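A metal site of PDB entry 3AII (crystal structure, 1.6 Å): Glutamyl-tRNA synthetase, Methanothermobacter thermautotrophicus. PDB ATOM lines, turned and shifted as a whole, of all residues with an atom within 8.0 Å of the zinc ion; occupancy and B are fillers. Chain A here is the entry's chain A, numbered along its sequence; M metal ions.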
ATOM      1  N   TYR A 189     -20.786   7.196  14.412  1.00  0.00           N
ATOM      2  CA  TYR A 189     -21.692   6.125  14.034  1.00  0.00           C
ATOM      3  C   TYR A 189     -20.940   4.996  13.375  1.00  0.00           C
ATOM      4  O   TYR A 189     -19.822   5.197  12.884  1.00  0.00           O
ATOM      5  CB  TYR A 189     -22.814   6.638  13.123  1.00  0.00           C
ATOM      6  CG  TYR A 189     -22.390   7.282  11.827  1.00  0.00           C
ATOM      7  CD1 TYR A 189     -21.907   8.590  11.784  1.00  0.00           C
ATOM      8  CD2 TYR A 189     -22.486   6.588  10.623  1.00  0.00           C
ATOM      9  CE1 TYR A 189     -21.542   9.180  10.591  1.00  0.00           C
ATOM     10  CE2 TYR A 189     -22.144   7.180   9.428  1.00  0.00           C
ATOM     11  CZ  TYR A 189     -21.671   8.460   9.413  1.00  0.00           C
ATOM     12  OH  TYR A 189     -21.311   9.024   8.203  1.00  0.00           O
ATOM     13  N   VAL A 190     -21.524   3.800  13.377  1.00  0.00           N
ATOM     14  CA  VAL A 190     -20.915   2.672  12.668  1.00  0.00           C
ATOM     15  C   VAL A 190     -21.497   2.539  11.281  1.00  0.00           C
ATOM     16  O   VAL A 190     -22.695   2.281  11.124  1.00  0.00           O
ATOM     17  CB  VAL A 190     -21.077   1.360  13.413  1.00  0.00           C
ATOM     18  CG1 VAL A 190     -20.377   0.236  12.630  1.00  0.00           C
ATOM     19  CG2 VAL A 190     -20.496   1.475  14.828  1.00  0.00           C
ATOM     20  N   CYS A 191     -20.645   2.720  10.283  1.00  0.00           N
ATOM     21  CA  CYS A 191     -21.084   2.703   8.892  1.00  0.00           C
ATOM     22  C   CYS A 191     -20.724   1.379   8.244  1.00  0.00           C
ATOM     23  O   CYS A 191     -19.558   0.989   8.199  1.00  0.00           O
ATOM     24  CB  CYS A 191     -20.432   3.845   8.115  1.00  0.00           C
ATOM     25  SG  CYS A 191     -20.983   3.925   6.396  1.00  0.00           S
ATOM     26  N   THR A 192     -21.760   0.720   7.726  1.00  0.00           N
ATOM     27  CA  THR A 192     -21.617  -0.565   7.066  1.00  0.00           C
ATOM     28  C   THR A 192     -21.765  -0.431   5.542  1.00  0.00           C
ATOM     29  O   THR A 192     -21.842  -1.440   4.842  1.00  0.00           O
ATOM     30  CB  THR A 192     -22.681  -1.552   7.569  1.00  0.00           C
ATOM     31  OG1 THR A 192     -23.972  -0.926   7.507  1.00  0.00           O
ATOM     32  CG2 THR A 192     -22.396  -1.963   9.008  1.00  0.00           C
ATOM     33  N   CYS A 193     -21.822   0.808   5.049  1.00  0.00           N
ATOM     34  CA  CYS A 193     -21.943   1.060   3.617  1.00  0.00           C
ATOM     35  C   CYS A 193     -20.721   0.580   2.856  1.00  0.00           C
ATOM     36  O   CYS A 193     -19.618   0.552   3.401  1.00  0.00           O
ATOM     37  CB  CYS A 193     -22.103   2.560   3.336  1.00  0.00           C
ATOM     38  SG  CYS A 193     -23.666   3.290   3.915  1.00  0.00           S
ATOM     39  N   ARG A 194     -20.908   0.219   1.594  1.00  0.00           N
ATOM     40  CA  ARG A 194     -19.771  -0.028   0.723  1.00  0.00           C
ATOM     41  C   ARG A 194     -19.073   1.304   0.536  1.00  0.00           C
ATOM     42  O   ARG A 194     -19.719   2.307   0.221  1.00  0.00           O
ATOM     43  CB  ARG A 194     -20.249  -0.571  -0.634  1.00  0.00           C
ATOM     44  CG  ARG A 194     -21.163  -1.787  -0.514  1.00  0.00           C
ATOM     45  CD  ARG A 194     -20.460  -2.972   0.112  1.00  0.00           C
ATOM     46  NE  ARG A 194     -21.396  -3.878   0.782  1.00  0.00           N
ATOM     47  CZ  ARG A 194     -21.093  -5.111   1.191  1.00  0.00           C
ATOM     48  NH1 ARG A 194     -19.879  -5.601   1.001  1.00  0.00           N
ATOM     49  NH2 ARG A 194     -22.016  -5.852   1.784  1.00  0.00           N
ATOM     50  N   GLU A 197     -20.012   3.609  -2.434  1.00  0.00           N
ATOM     51  CA  GLU A 197     -21.379   4.118  -2.351  1.00  0.00           C
ATOM     52  C   GLU A 197     -21.462   5.220  -1.305  1.00  0.00           C
ATOM     53  O   GLU A 197     -22.141   6.224  -1.498  1.00  0.00           O
ATOM     54  CB  GLU A 197     -22.361   2.983  -2.052  1.00  0.00           C
ATOM     55  CG  GLU A 197     -23.727   3.183  -2.708  1.00  0.00           C
ATOM     56  CD  GLU A 197     -24.874   3.102  -1.732  1.00  0.00           C
ATOM     57  OE1 GLU A 197     -25.026   2.059  -1.066  1.00  0.00           O
ATOM     58  OE2 GLU A 197     -25.645   4.085  -1.637  1.00  0.00           O
ATOM     59  N   PHE A 198     -20.772   5.024  -0.184  1.00  0.00           N
ATOM     60  CA  PHE A 198     -20.694   6.071   0.835  1.00  0.00           C
ATOM     61  C   PHE A 198     -20.041   7.327   0.289  1.00  0.00           C
ATOM     62  O   PHE A 198     -20.494   8.439   0.555  1.00  0.00           O
ATOM     63  CB  PHE A 198     -19.926   5.597   2.077  1.00  0.00           C
ATOM     64  CG  PHE A 198     -19.895   6.626   3.173  1.00  0.00           C
ATOM     65  CD1 PHE A 198     -18.843   7.538   3.256  1.00  0.00           C
ATOM     66  CD2 PHE A 198     -20.930   6.720   4.085  1.00  0.00           C
ATOM     67  CE1 PHE A 198     -18.831   8.508   4.230  1.00  0.00           C
ATOM     68  CE2 PHE A 198     -20.918   7.690   5.060  1.00  0.00           C
ATOM     69  CZ  PHE A 198     -19.864   8.581   5.146  1.00  0.00           C
ATOM     70  N   LEU A 201     -22.330   9.497  -1.838  1.00  0.00           N
ATOM     71  CA  LEU A 201     -23.268  10.260  -1.004  1.00  0.00           C
ATOM     72  C   LEU A 201     -22.555  11.423  -0.346  1.00  0.00           C
ATOM     73  O   LEU A 201     -23.010  12.570  -0.399  1.00  0.00           O
ATOM     74  CB  LEU A 201     -23.903   9.361   0.058  1.00  0.00           C
ATOM     75  CG  LEU A 201     -24.904   8.312  -0.412  1.00  0.00           C
ATOM     76  CD1 LEU A 201     -25.297   7.393   0.737  1.00  0.00           C
ATOM     77  CD2 LEU A 201     -26.132   8.981  -1.032  1.00  0.00           C
ATOM     78  N   ALA A 207     -26.445  12.198   3.564  1.00  0.00           N
ATOM     79  CA  ALA A 207     -26.168  11.234   4.633  1.00  0.00           C
ATOM     80  C   ALA A 207     -26.570   9.818   4.254  1.00  0.00           C
ATOM     81  O   ALA A 207     -27.571   9.609   3.560  1.00  0.00           O
ATOM     82  CB  ALA A 207     -26.875  11.652   5.912  1.00  0.00           C
ATOM     83  N   CYS A 208     -25.787   8.844   4.695  1.00  0.00           N
ATOM     84  CA  CYS A 208     -26.155   7.456   4.544  1.00  0.00           C
ATOM     85  C   CYS A 208     -27.142   7.117   5.662  1.00  0.00           C
ATOM     86  O   CYS A 208     -27.345   7.909   6.582  1.00  0.00           O
ATOM     87  CB  CYS A 208     -24.930   6.534   4.607  1.00  0.00           C
ATOM     88  SG  CYS A 208     -24.197   6.395   6.268  1.00  0.00           S
ATOM     89  N   HIS A 209     -27.753   5.941   5.558  1.00  0.00           N
ATOM     90  CA  HIS A 209     -28.713   5.507   6.562  1.00  0.00           C
ATOM     91  C   HIS A 209     -28.073   5.356   7.945  1.00  0.00           C
ATOM     92  O   HIS A 209     -28.725   5.611   8.970  1.00  0.00           O
ATOM     93  CB  HIS A 209     -29.347   4.184   6.126  1.00  0.00           C
ATOM     94  CG  HIS A 209     -30.138   3.508   7.209  1.00  0.00           C
ATOM     95  ND1 HIS A 209     -31.348   3.989   7.659  1.00  0.00           N
ATOM     96  CD2 HIS A 209     -29.892   2.393   7.926  1.00  0.00           C
ATOM     97  CE1 HIS A 209     -31.813   3.193   8.605  1.00  0.00           C
ATOM     98  NE2 HIS A 209     -30.945   2.218   8.797  1.00  0.00           N
ATOM     99  N   CYS A 210     -26.805   4.957   7.983  1.00  0.00           N
ATOM    100  CA  CYS A 210     -26.129   4.661   9.244  1.00  0.00           C
ATOM    101  C   CYS A 210     -26.078   5.911  10.134  1.00  0.00           C
ATOM    102  O   CYS A 210     -26.084   5.817  11.360  1.00  0.00           O
ATOM    103  CB  CYS A 210     -24.701   4.179   8.971  1.00  0.00           C
ATOM    104  SG  CYS A 210     -24.554   2.895   7.695  1.00  0.00           S
ATOM    105  N   ARG A 211     -26.007   7.069   9.485  1.00  0.00           N
ATOM    106  CA  ARG A 211     -25.838   8.329  10.195  1.00  0.00           C
ATOM    107  C   ARG A 211     -27.050   8.683  11.036  1.00  0.00           C
ATOM    108  O   ARG A 211     -26.964   9.550  11.911  1.00  0.00           O
ATOM    109  CB  ARG A 211     -25.555   9.452   9.200  1.00  0.00           C
ATOM    110  CG  ARG A 211     -24.770  10.618   9.790  1.00  0.00           C
ATOM    111  CD  ARG A 211     -24.676  11.764   8.800  1.00  0.00           C
ATOM    112  NE  ARG A 211     -23.525  12.635   9.046  1.00  0.00           N
ATOM    113  CZ  ARG A 211     -23.570  13.779   9.740  1.00  0.00           C
ATOM    114  NH1 ARG A 211     -24.710  14.202  10.269  1.00  0.00           N
ATOM    115  NH2 ARG A 211     -22.466  14.490   9.899  1.00  0.00           N
ATOM    116  N   SER A 212     -28.178   8.021  10.779  1.00  0.00           N
ATOM    117  CA  SER A 212     -29.415   8.313  11.511  1.00  0.00           C
ATOM    118  C   SER A 212     -29.677   7.361  12.671  1.00  0.00           C
ATOM    119  O   SER A 212     -30.646   7.539  13.409  1.00  0.00           O
ATOM    120  CB  SER A 212     -30.617   8.294  10.547  1.00  0.00           C
ATOM    121  OG  SER A 212     -30.888   6.972  10.096  1.00  0.00           O
ATOM    122  N   LEU A 213     -28.831   6.346  12.826  1.00  0.00           N
ATOM    123  CA  LEU A 213     -29.027   5.362  13.899  1.00  0.00           C
ATOM    124  C   LEU A 213     -28.884   6.008  15.270  1.00  0.00           C
ATOM    125  O   LEU A 213     -28.150   6.978  15.447  1.00  0.00           O
ATOM    126  CB  LEU A 213     -28.027   4.203  13.782  1.00  0.00           C
ATOM    127  CG  LEU A 213     -28.073   3.421  12.469  1.00  0.00           C
ATOM    128  CD1 LEU A 213     -26.993   2.348  12.471  1.00  0.00           C
ATOM    129  CD2 LEU A 213     -29.442   2.797  12.284  1.00  0.00           C
ATOM    130  N   ARG A 221     -23.761  -2.297  16.661  1.00  0.00           N
ATOM    131  CA  ARG A 221     -22.923  -2.428  15.477  1.00  0.00           C
ATOM    132  C   ARG A 221     -21.444  -2.334  15.862  1.00  0.00           C
ATOM    133  O   ARG A 221     -20.601  -3.024  15.280  1.00  0.00           O
ATOM    134  CB  ARG A 221     -23.212  -1.316  14.477  1.00  0.00           C
ATOM    135  CG  ARG A 221     -24.565  -1.427  13.780  1.00  0.00           C
ATOM    136  CD  ARG A 221     -24.557  -0.489  12.583  1.00  0.00           C
ATOM    137  NE  ARG A 221     -25.708  -0.658  11.699  1.00  0.00           N
ATOM    138  CZ  ARG A 221     -25.807  -0.088  10.507  1.00  0.00           C
ATOM    139  NH1 ARG A 221     -24.831   0.690  10.071  1.00  0.00           N
ATOM    140  NH2 ARG A 221     -26.881  -0.286   9.753  1.00  0.00           N
ATOM    141  N   VAL A 234     -16.689   0.564   9.413  1.00  0.00           N
ATOM    142  CA  VAL A 234     -15.837   1.554  10.060  1.00  0.00           C
ATOM    143  C   VAL A 234     -16.669   2.377  11.030  1.00  0.00           C
ATOM    144  O   VAL A 234     -17.909   2.429  10.924  1.00  0.00           O
ATOM    145  CB  VAL A 234     -15.159   2.482   9.036  1.00  0.00           C
ATOM    146  CG1 VAL A 234     -14.130   1.698   8.218  1.00  0.00           C
ATOM    147  CG2 VAL A 234     -16.210   3.124   8.127  1.00  0.00           C
ATOM    148  N   ARG A 236     -17.276   6.234  11.896  1.00  0.00           N
ATOM    149  CA  ARG A 236     -17.087   7.570  11.326  1.00  0.00           C
ATOM    150  C   ARG A 236     -17.470   8.644  12.325  1.00  0.00           C
ATOM    151  O   ARG A 236     -18.466   8.513  13.024  1.00  0.00           O
ATOM    152  CB  ARG A 236     -17.930   7.724  10.058  1.00  0.00           C
ATOM    153  CG  ARG A 236     -17.458   6.835   8.930  1.00  0.00           C
ATOM    154  CD  ARG A 236     -18.309   7.017   7.673  1.00  0.00           C
ATOM    155  NE  ARG A 236     -17.754   6.218   6.576  1.00  0.00           N
ATOM    156  CZ  ARG A 236     -16.696   6.579   5.856  1.00  0.00           C
ATOM    157  NH1 ARG A 236     -16.067   7.713   6.107  1.00  0.00           N
ATOM    158  NH2 ARG A 236     -16.258   5.796   4.881  1.00  0.00           N
HETATM  159 ZN    ZN M   1     -23.304   4.134   6.104  1.00  0.00          ZN
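The backbone NH (N) of Cys 191 is in hydrogen-bond range of the backbone carbonyl oxygen (O) of Val 234 (2.8 Å). The side-chain sulfur of Cys 210 lies close to the backbone NH of Thr 192, 3.5 Å away. The side-chain sulfur (SG) of Cys 210 lies close to the guanidinium group (NH1) of Arg 221 (3.3 Å). N of Arg 211 lies close to SG of Cys 208, 3.8 Å away.
Within 4 Å of the zinc ion: Cys 191, Cys 193, Cys 208 and Cys 210. The nearest printed residue that does not touch the zinc ion is Phe 198 (4.05 Å).
The zinc ion is bound by SG of Cys 191 (2.3 Å), SG of Cys 210 (2.4 Å), SG of Cys 193 (2.4 Å) and SG of Cys 208 (2.4 Å). The zinc ion has four donor atoms within binding distance.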
